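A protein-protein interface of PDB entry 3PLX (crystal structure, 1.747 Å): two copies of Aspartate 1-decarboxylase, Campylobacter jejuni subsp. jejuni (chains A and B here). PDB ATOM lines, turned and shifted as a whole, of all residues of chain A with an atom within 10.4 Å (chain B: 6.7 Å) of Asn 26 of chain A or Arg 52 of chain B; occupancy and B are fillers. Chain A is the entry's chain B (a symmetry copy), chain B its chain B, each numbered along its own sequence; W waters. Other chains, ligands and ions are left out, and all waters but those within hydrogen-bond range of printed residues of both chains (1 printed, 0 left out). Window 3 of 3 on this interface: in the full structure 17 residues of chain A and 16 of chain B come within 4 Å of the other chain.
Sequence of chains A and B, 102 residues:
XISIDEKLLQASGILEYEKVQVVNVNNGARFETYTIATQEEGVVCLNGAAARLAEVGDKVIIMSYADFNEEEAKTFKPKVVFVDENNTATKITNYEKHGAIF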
ATOM      1  N   VAL A  22      -6.289 -21.628 -13.968  1.00  0.00           N
ATOM      2  CA  VAL A  22      -7.219 -21.354 -12.876  1.00  0.00           C
ATOM      3  C   VAL A  22      -6.415 -20.662 -11.786  1.00  0.00           C
ATOM      4  O   VAL A  22      -5.350 -21.147 -11.398  1.00  0.00           O
ATOM      5  CB  VAL A  22      -7.803 -22.665 -12.312  1.00  0.00           C
ATOM      6  CG1 VAL A  22      -8.800 -22.353 -11.184  1.00  0.00           C
ATOM      7  CG2 VAL A  22      -8.454 -23.478 -13.420  1.00  0.00           C
ATOM      8  N   VAL A  23      -6.900 -19.521 -11.303  1.00  0.00           N
ATOM      9  CA  VAL A  23      -6.213 -18.855 -10.196  1.00  0.00           C
ATOM     10  C   VAL A  23      -7.209 -18.635  -9.072  1.00  0.00           C
ATOM     11  O   VAL A  23      -8.393 -18.400  -9.308  1.00  0.00           O
ATOM     12  CB  VAL A  23      -5.514 -17.536 -10.626  1.00  0.00           C
ATOM     13  CG1 VAL A  23      -4.540 -17.808 -11.778  1.00  0.00           C
ATOM     14  CG2 VAL A  23      -6.540 -16.501 -11.046  1.00  0.00           C
ATOM     15  N   ASN A  24      -6.721 -18.774  -7.846  1.00  0.00           N
ATOM     16  CA  ASN A  24      -7.572 -18.773  -6.673  1.00  0.00           C
ATOM     17  C   ASN A  24      -7.318 -17.466  -5.939  1.00  0.00           C
ATOM     18  O   ASN A  24      -6.214 -17.219  -5.466  1.00  0.00           O
ATOM     19  CB  ASN A  24      -7.228 -19.995  -5.812  1.00  0.00           C
ATOM     20  CG  ASN A  24      -8.117 -20.143  -4.600  1.00  0.00           C
ATOM     21  OD1 ASN A  24      -8.568 -19.159  -4.025  1.00  0.00           O
ATOM     22  ND2 ASN A  24      -8.342 -21.400  -4.176  1.00  0.00           N
ATOM     23  N   VAL A  25      -8.341 -16.617  -5.885  1.00  0.00           N
ATOM     24  CA  VAL A  25      -8.226 -15.318  -5.240  1.00  0.00           C
ATOM     25  C   VAL A  25      -7.991 -15.441  -3.740  1.00  0.00           C
ATOM     26  O   VAL A  25      -7.259 -14.639  -3.150  1.00  0.00           O
ATOM     27  CB  VAL A  25      -9.472 -14.450  -5.511  1.00  0.00           C
ATOM     28  CG1 VAL A  25      -9.310 -13.084  -4.889  1.00  0.00           C
ATOM     29  CG2 VAL A  25      -9.670 -14.315  -7.020  1.00  0.00           C
ATOM     30  N   ASN A  26      -8.600 -16.449  -3.119  1.00  0.00           N
ATOM     31  CA  ASN A  26      -8.441 -16.622  -1.679  1.00  0.00           C
ATOM     32  C   ASN A  26      -7.018 -16.975  -1.248  1.00  0.00           C
ATOM     33  O   ASN A  26      -6.509 -16.411  -0.283  1.00  0.00           O
ATOM     34  CB  ASN A  26      -9.401 -17.687  -1.131  1.00  0.00           C
ATOM     35  CG  ASN A  26     -10.848 -17.284  -1.262  1.00  0.00           C
ATOM     36  OD1 ASN A  26     -11.312 -16.938  -2.347  1.00  0.00           O
ATOM     37  ND2 ASN A  26     -11.572 -17.326  -0.154  1.00  0.00           N
ATOM     38  N   ASN A  27      -6.382 -17.921  -1.936  1.00  0.00           N
ATOM     39  CA  ASN A  27      -5.071 -18.395  -1.482  1.00  0.00           C
ATOM     40  C   ASN A  27      -3.912 -18.106  -2.438  1.00  0.00           C
ATOM     41  O   ASN A  27      -2.753 -18.433  -2.135  1.00  0.00           O
ATOM     42  CB  ASN A  27      -5.117 -19.901  -1.145  1.00  0.00           C
ATOM     43  CG  ASN A  27      -5.301 -20.768  -2.380  1.00  0.00           C
ATOM     44  OD1 ASN A  27      -5.279 -20.273  -3.499  1.00  0.00           O
ATOM     45  ND2 ASN A  27      -5.520 -22.068  -2.174  1.00  0.00           N
ATOM     46  N   GLY A  28      -4.218 -17.481  -3.571  1.00  0.00           N
ATOM     47  CA  GLY A  28      -3.186 -17.103  -4.522  1.00  0.00           C
ATOM     48  C   GLY A  28      -2.648 -18.217  -5.389  1.00  0.00           C
ATOM     49  O   GLY A  28      -1.703 -18.014  -6.173  1.00  0.00           O
ATOM     50  N   ALA A  29      -3.210 -19.415  -5.254  1.00  0.00           N
ATOM     51  CA  ALA A  29      -2.733 -20.522  -6.080  1.00  0.00           C
ATOM     52  C   ALA A  29      -2.993 -20.235  -7.556  1.00  0.00           C
ATOM     53  O   ALA A  29      -3.985 -19.597  -7.912  1.00  0.00           O
ATOM     54  CB  ALA A  29      -3.393 -21.854  -5.676  1.00  0.00           C
ATOM     55  N   ARG A  30      -2.104 -20.742  -8.412  1.00  0.00           N
ATOM     56  CA  ARG A  30      -2.243 -20.604  -9.870  1.00  0.00           C
ATOM     57  C   ARG A  30      -1.839 -21.923 -10.498  1.00  0.00           C
ATOM     58  O   ARG A  30      -0.771 -22.451 -10.199  1.00  0.00           O
ATOM     59  CB  ARG A  30      -1.316 -19.493 -10.398  1.00  0.00           C
ATOM     60  CG  ARG A  30      -1.472 -18.159  -9.644  1.00  0.00           C
ATOM     61  CD  ARG A  30      -0.514 -17.088 -10.194  1.00  0.00           C
ATOM     62  NE  ARG A  30      -0.971 -16.510 -11.464  1.00  0.00           N
ATOM     63  CZ  ARG A  30      -1.892 -15.553 -11.557  1.00  0.00           C
ATOM     64  NH1 ARG A  30      -2.478 -15.081 -10.459  1.00  0.00           N
ATOM     65  NH2 ARG A  30      -2.246 -15.070 -12.751  1.00  0.00           N
ATOM     66  N   PHE A  31      -2.684 -22.462 -11.373  1.00  0.00           N
ATOM     67  CA  PHE A  31      -2.382 -23.742 -11.997  1.00  0.00           C
ATOM     68  C   PHE A  31      -3.050 -23.887 -13.348  1.00  0.00           C
ATOM     69  O   PHE A  31      -3.945 -23.108 -13.706  1.00  0.00           O
ATOM     70  CB  PHE A  31      -2.761 -24.923 -11.070  1.00  0.00           C
ATOM     71  CG  PHE A  31      -4.232 -25.005 -10.712  1.00  0.00           C
ATOM     72  CD1 PHE A  31      -5.076 -25.887 -11.369  1.00  0.00           C
ATOM     73  CD2 PHE A  31      -4.752 -24.235  -9.680  1.00  0.00           C
ATOM     74  CE1 PHE A  31      -6.434 -25.975 -11.034  1.00  0.00           C
ATOM     75  CE2 PHE A  31      -6.102 -24.322  -9.337  1.00  0.00           C
ATOM     76  CZ  PHE A  31      -6.944 -25.194 -10.021  1.00  0.00           C
ATOM     77  N   LEU A  53      -5.609 -27.385  -3.958  1.00  0.00           N
ATOM     78  CA  LEU A  53      -5.338 -25.970  -4.197  1.00  0.00           C
ATOM     79  C   LEU A  53      -6.556 -25.077  -3.982  1.00  0.00           C
ATOM     80  O   LEU A  53      -6.519 -23.880  -4.279  1.00  0.00           O
ATOM     81  CB  LEU A  53      -4.802 -25.780  -5.618  1.00  0.00           C
ATOM     82  CG  LEU A  53      -3.515 -26.559  -5.887  1.00  0.00           C
ATOM     83  CD1 LEU A  53      -3.083 -26.301  -7.325  1.00  0.00           C
ATOM     84  CD2 LEU A  53      -2.421 -26.175  -4.905  1.00  0.00           C
ATOM     85  N   ALA A  54      -7.639 -25.650  -3.470  1.00  0.00           N
ATOM     86  CA  ALA A  54      -8.798 -24.830  -3.136  1.00  0.00           C
ATOM     87  C   ALA A  54      -9.670 -25.488  -2.087  1.00  0.00           C
ATOM     88  O   ALA A  54      -9.601 -26.697  -1.873  1.00  0.00           O
ATOM     89  CB  ALA A  54      -9.623 -24.524  -4.379  1.00  0.00           C
ATOM     90  N   GLU A  55     -10.492 -24.672  -1.436  1.00  0.00           N
ATOM     91  CA  GLU A  55     -11.509 -25.156  -0.508  1.00  0.00           C
ATOM     92  C   GLU A  55     -12.856 -24.670  -1.024  1.00  0.00           C
ATOM     93  O   GLU A  55     -12.925 -23.680  -1.752  1.00  0.00           O
ATOM     94  CB  GLU A  55     -11.264 -24.614   0.897  1.00  0.00           C
ATOM     95  CG  GLU A  55      -9.945 -25.107   1.483  1.00  0.00           C
ATOM     96  CD  GLU A  55      -9.976 -26.602   1.750  1.00  0.00           C
ATOM     97  OE1 GLU A  55     -11.018 -27.081   2.233  1.00  0.00           O
ATOM     98  OE2 GLU A  55      -8.965 -27.292   1.476  1.00  0.00           O
ATOM     99  N   VAL A  56     -13.917 -25.378  -0.665  1.00  0.00           N
ATOM    100  CA  VAL A  56     -15.255 -24.947  -1.054  1.00  0.00           C
ATOM    101  C   VAL A  56     -15.478 -23.503  -0.627  1.00  0.00           C
ATOM    102  O   VAL A  56     -15.199 -23.136   0.514  1.00  0.00           O
ATOM    103  CB  VAL A  56     -16.328 -25.819  -0.388  1.00  0.00           C
ATOM    104  CG1 VAL A  56     -17.725 -25.268  -0.700  1.00  0.00           C
ATOM    105  CG2 VAL A  56     -16.196 -27.258  -0.848  1.00  0.00           C
ATOM    106  N   GLY A  57     -15.988 -22.684  -1.542  1.00  0.00           N
ATOM    107  CA  GLY A  57     -16.239 -21.285  -1.254  1.00  0.00           C
ATOM    108  C   GLY A  57     -15.196 -20.345  -1.829  1.00  0.00           C
ATOM    109  O   GLY A  57     -15.449 -19.151  -1.948  1.00  0.00           O
ATOM    110  N   ASP A  58     -14.020 -20.868  -2.176  1.00  0.00           N
ATOM    111  CA  ASP A  58     -12.963 -20.011  -2.730  1.00  0.00           C
ATOM    112  C   ASP A  58     -13.411 -19.389  -4.046  1.00  0.00           C
ATOM    113  O   ASP A  58     -14.149 -20.002  -4.811  1.00  0.00           O
ATOM    114  CB  ASP A  58     -11.680 -20.805  -2.980  1.00  0.00           C
ATOM    115  CG  ASP A  58     -10.930 -21.147  -1.694  1.00  0.00           C
ATOM    116  OD1 ASP A  58     -11.345 -20.698  -0.591  1.00  0.00           O
ATOM    117  OD2 ASP A  58      -9.919 -21.876  -1.796  1.00  0.00           O
ATOM    118  N   LYS A  59     -12.956 -18.171  -4.304  1.00  0.00           N
ATOM    119  CA  LYS A  59     -13.256 -17.498  -5.561  1.00  0.00           C
ATOM    120  C   LYS A  59     -12.125 -17.791  -6.535  1.00  0.00           C
ATOM    121  O   LYS A  59     -10.955 -17.609  -6.206  1.00  0.00           O
ATOM    122  CB  LYS A  59     -13.383 -15.993  -5.332  1.00  0.00           C
ATOM    123  CG  LYS A  59     -14.609 -15.589  -4.506  1.00  0.00           C
ATOM    124  CD  LYS A  59     -15.878 -15.859  -5.301  1.00  0.00           C
ATOM    125  CE  LYS A  59     -17.106 -15.210  -4.682  1.00  0.00           C
ATOM    126  NZ  LYS A  59     -17.470 -15.841  -3.395  1.00  0.00           N
ATOM    127  N   VAL A  60     -12.477 -18.260  -7.726  1.00  0.00           N
ATOM    128  CA  VAL A  60     -11.480 -18.568  -8.751  1.00  0.00           C
ATOM    129  C   VAL A  60     -11.759 -17.816 -10.046  1.00  0.00           C
ATOM    130  O   VAL A  60     -12.894 -17.442 -10.333  1.00  0.00           O
ATOM    131  CB  VAL A  60     -11.387 -20.090  -9.060  1.00  0.00           C
ATOM    132  CG1 VAL A  60     -10.885 -20.877  -7.829  1.00  0.00           C
ATOM    133  CG2 VAL A  60     -12.732 -20.647  -9.538  1.00  0.00           C
ATOM    134  N   ILE A  61     -10.698 -17.581 -10.809  1.00  0.00           N
ATOM    135  CA  ILE A  61     -10.806 -16.977 -12.123  1.00  0.00           C
ATOM    136  C   ILE A  61     -10.258 -18.022 -13.092  1.00  0.00           C
ATOM    137  O   ILE A  61      -9.157 -18.543 -12.889  1.00  0.00           O
ATOM    138  CB  ILE A  61     -10.007 -15.660 -12.186  1.00  0.00           C
ATOM    139  CG1 ILE A  61     -10.590 -14.663 -11.169  1.00  0.00           C
ATOM    140  CG2 ILE A  61     -10.037 -15.074 -13.601  1.00  0.00           C
ATOM    141  CD1 ILE A  61      -9.753 -13.431 -10.956  1.00  0.00           C
ATOM    142  N   ASN B  27      10.522 -10.757  -4.377  1.00  0.00           N
ATOM    143  CA  ASN B  27      10.141 -11.988  -3.679  1.00  0.00           C
ATOM    144  C   ASN B  27      10.320 -13.273  -4.489  1.00  0.00           C
ATOM    145  O   ASN B  27      10.060 -14.376  -3.980  1.00  0.00           O
ATOM    146  CB  ASN B  27       8.694 -11.893  -3.148  1.00  0.00           C
ATOM    147  CG  ASN B  27       7.664 -11.890  -4.265  1.00  0.00           C
ATOM    148  OD1 ASN B  27       8.002 -12.075  -5.427  1.00  0.00           O
ATOM    149  ND2 ASN B  27       6.400 -11.644  -3.915  1.00  0.00           N
ATOM    150  N   LEU B  46      -1.354  -4.944 -10.057  1.00  0.00           N
ATOM    151  CA  LEU B  46      -1.707  -6.361 -10.084  1.00  0.00           C
ATOM    152  C   LEU B  46      -3.084  -6.578  -9.479  1.00  0.00           C
ATOM    153  O   LEU B  46      -3.306  -6.287  -8.313  1.00  0.00           O
ATOM    154  CB  LEU B  46      -0.657  -7.206  -9.359  1.00  0.00           C
ATOM    155  CG  LEU B  46       0.663  -7.357 -10.112  1.00  0.00           C
ATOM    156  CD1 LEU B  46       1.690  -8.040  -9.246  1.00  0.00           C
ATOM    157  CD2 LEU B  46       0.453  -8.128 -11.406  1.00  0.00           C
ATOM    158  N   ASN B  47      -4.004  -7.095 -10.293  1.00  0.00           N
ATOM    159  CA  ASN B  47      -5.384  -7.314  -9.878  1.00  0.00           C
ATOM    160  C   ASN B  47      -5.642  -8.782  -9.606  1.00  0.00           C
ATOM    161  O   ASN B  47      -4.918  -9.642 -10.104  1.00  0.00           O
ATOM    162  CB  ASN B  47      -6.340  -6.896 -10.996  1.00  0.00           C
ATOM    163  CG  ASN B  47      -6.072  -5.498 -11.500  1.00  0.00           C
ATOM    164  OD1 ASN B  47      -6.243  -4.519 -10.768  1.00  0.00           O
ATOM    165  ND2 ASN B  47      -5.661  -5.391 -12.764  1.00  0.00           N
ATOM    166  N   GLY B  48      -6.704  -9.069  -8.860  1.00  0.00           N
ATOM    167  CA  GLY B  48      -7.111 -10.449  -8.638  1.00  0.00           C
ATOM    168  C   GLY B  48      -6.119 -11.271  -7.838  1.00  0.00           C
ATOM    169  O   GLY B  48      -5.477 -10.765  -6.920  1.00  0.00           O
ATOM    170  N   ALA B  49      -5.999 -12.549  -8.178  1.00  0.00           N
ATOM    171  CA  ALA B  49      -5.155 -13.452  -7.413  1.00  0.00           C
ATOM    172  C   ALA B  49      -3.703 -12.980  -7.422  1.00  0.00           C
ATOM    173  O   ALA B  49      -2.966 -13.204  -6.456  1.00  0.00           O
ATOM    174  CB  ALA B  49      -5.266 -14.885  -7.948  1.00  0.00           C
ATOM    175  N   ALA B  50      -3.295 -12.329  -8.510  1.00  0.00           N
ATOM    176  CA  ALA B  50      -1.913 -11.862  -8.637  1.00  0.00           C
ATOM    177  C   ALA B  50      -1.549 -10.844  -7.556  1.00  0.00           C
ATOM    178  O   ALA B  50      -0.373 -10.634  -7.252  1.00  0.00           O
ATOM    179  CB  ALA B  50      -1.665 -11.283 -10.015  1.00  0.00           C
ATOM    180  N   ALA B  51      -2.561 -10.225  -6.961  1.00  0.00           N
ATOM    181  CA  ALA B  51      -2.310  -9.254  -5.895  1.00  0.00           C
ATOM    182  C   ALA B  51      -1.552  -9.881  -4.735  1.00  0.00           C
ATOM    183  O   ALA B  51      -0.839  -9.189  -4.006  1.00  0.00           O
ATOM    184  CB  ALA B  51      -3.636  -8.651  -5.397  1.00  0.00           C
ATOM    185  N   ARG B  52      -1.723 -11.187  -4.540  1.00  0.00           N
ATOM    186  CA  ARG B  52      -1.026 -11.868  -3.451  1.00  0.00           C
ATOM    187  C   ARG B  52       0.445 -12.145  -3.743  1.00  0.00           C
ATOM    188  O   ARG B  52       1.168 -12.666  -2.880  1.00  0.00           O
ATOM    189  CB  ARG B  52      -1.730 -13.179  -3.120  1.00  0.00           C
ATOM    190  CG  ARG B  52      -3.116 -12.942  -2.556  1.00  0.00           C
ATOM    191  CD  ARG B  52      -3.757 -14.219  -2.043  1.00  0.00           C
ATOM    192  NE  ARG B  52      -5.113 -13.955  -1.556  1.00  0.00           N
ATOM    193  CZ  ARG B  52      -5.395 -13.508  -0.335  1.00  0.00           C
ATOM    194  NH1 ARG B  52      -4.413 -13.280   0.535  1.00  0.00           N
ATOM    195  NH2 ARG B  52      -6.649 -13.286   0.016  1.00  0.00           N
ATOM    196  N   LEU B  53       0.888 -11.815  -4.945  1.00  0.00           N
ATOM    197  CA  LEU B  53       2.263 -12.118  -5.335  1.00  0.00           C
ATOM    198  C   LEU B  53       3.152 -10.881  -5.422  1.00  0.00           C
ATOM    199  O   LEU B  53       4.299 -10.961  -5.873  1.00  0.00           O
ATOM    200  CB  LEU B  53       2.268 -12.854  -6.676  1.00  0.00           C
ATOM    201  CG  LEU B  53       1.485 -14.166  -6.649  1.00  0.00           C
ATOM    202  CD1 LEU B  53       1.554 -14.802  -8.031  1.00  0.00           C
ATOM    203  CD2 LEU B  53       2.022 -15.106  -5.581  1.00  0.00           C
ATOM    204  N   ALA B  54       2.633  -9.736  -4.997  1.00  0.00           N
ATOM    205  CA  ALA B  54       3.467  -8.540  -4.950  1.00  0.00           C
ATOM    206  C   ALA B  54       2.941  -7.525  -3.956  1.00  0.00           C
ATOM    207  O   ALA B  54       1.774  -7.562  -3.570  1.00  0.00           O
ATOM    208  CB  ALA B  54       3.585  -7.904  -6.328  1.00  0.00           C
ATOM    209  N   GLU B  55       3.821  -6.617  -3.548  1.00  0.00           N
ATOM    210  CA  GLU B  55       3.449  -5.477  -2.718  1.00  0.00           C
ATOM    211  C   GLU B  55       3.832  -4.219  -3.485  1.00  0.00           C
ATOM    212  O   GLU B  55       4.712  -4.256  -4.345  1.00  0.00           O
ATOM    213  CB  GLU B  55       4.182  -5.516  -1.381  1.00  0.00           C
ATOM    214  CG  GLU B  55       3.799  -6.735  -0.549  1.00  0.00           C
ATOM    215  CD  GLU B  55       2.354  -6.666  -0.087  1.00  0.00           C
ATOM    216  OE1 GLU B  55       1.925  -5.564   0.303  1.00  0.00           O
ATOM    217  OE2 GLU B  55       1.653  -7.706  -0.115  1.00  0.00           O
HETATM  218  O   HOH W   1      -1.908 -15.589  -7.594  1.00  0.00           O
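Water W1 lies within hydrogen-bond range of O of Gly 28 of chain A (2.8 Å), O of Ala 49 of chain B (2.8 Å) and NH1 of Arg 30 of chain A (3.0 Å).
Hydrophobic or aromatic side chains of chain B within 4 Å of the printed part of chain A: Ala 49, Ala 50 and Leu 53. Along chain B the printed residues that touch a printed residue of chain A span positions 49 to 53. Printed residues of chain A that touch a printed residue of chain B: Val 23, Asn 24, Val 25, Asn 26, Asn 27, Gly 28 and Arg 30. Along chain A the printed residues that touch a printed residue of chain B span positions 23 to 30. Among the printed residues, 9 pairs touch across the chains. Among the printed residues, no Asp or Glu carboxylate lies within 4 Å of a Lys or Arg side-chain nitrogen of the other chain.
The backbone carbonyl oxygen (O) of Val 25 of chain A is in hydrogen-bond range of the guanidinium group (NE) of Arg 52 of chain B, 2.8 Å away. O of Asn 26 of chain A lies within hydrogen-bond range of NE of Arg 52 of chain B (3.1 Å). N of Ala 50 of chain B lies close to NH1 of Arg 30 of chain A.
4 positions are printed for both chains.
Among the printed residues, merely in contact across the chains: Val 23 of chain A with Ala 49 of chain B, Asn 24 of chain A with Ala 49 of chain B, Asn 27 of chain A with Arg 52 of chain B, Gly 28 of chain A with Arg 52 of chain B, Arg 30 of chain A with Ala 49 of chain B and Arg 30 of chain A with Leu 53 of chain B.
N of Ile 61 of chain A lies within hydrogen-bond range of O of Val 23 of chain A, at 2.9 Å. The backbone NH (N) of Asn 27 of chain A sits at hydrogen-bond distance from the side-chain amide oxygen (OD1) of Asn 24 of chain A (3.3 Å). The side-chain amide nitrogen (ND2) of Asn 24 of chain A is in hydrogen-bond range of the backbone carbonyl oxygen (O) of Leu 53 of chain A, 3.1 Å away. The side-chain carboxylate (OD1) of Asp 58 of chain A is in hydrogen-bond range of the side-chain amide nitrogen (ND2) of Asn 26 of chain A, at 3.4 Å. The backbone NH of Lys 59 of chain A sits at hydrogen-bond distance from the side-chain amide oxygen of Asn 26 of chain A, 2.8 Å away. The backbone carbonyl oxygen of Leu 53 of chain A sits at hydrogen-bond distance from the side-chain amide nitrogen of Asn 27 of chain A.
Printed residues of chain B within 4 Å of Val 23 of chain A: Ala 49 (3.7 Å). Printed residues of chain B within 4 Å of Asn 24 of chain A: Ala 49 (3.5 Å). Printed residues of chain B within 4 Å of Arg 30 of chain A: Ala 49 (3.8 Å), Ala 50 (3.5 Å) and Leu 53 (3.8 Å). Ala 50 of chain B touches one residue of chain A. No residue of chain A comes within 4 Å of Ala 51 of chain B. Of chain A, only Val 25, Asn 26, Asn 27 and Gly 28 come within 4 Å of Arg 52 of chain B. Leu 53 of chain B touches one residue of chain A. No residue of chain A comes within 4 Å of Ala 54 of chain B. The nearest residue of chain B that does not touch Asn 26 of chain A is Ala 49 of chain B (6.1 Å). The nearest printed residue of chain B that does not touch Val 23 of chain A is Ala 50 of chain B (5.9 Å).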
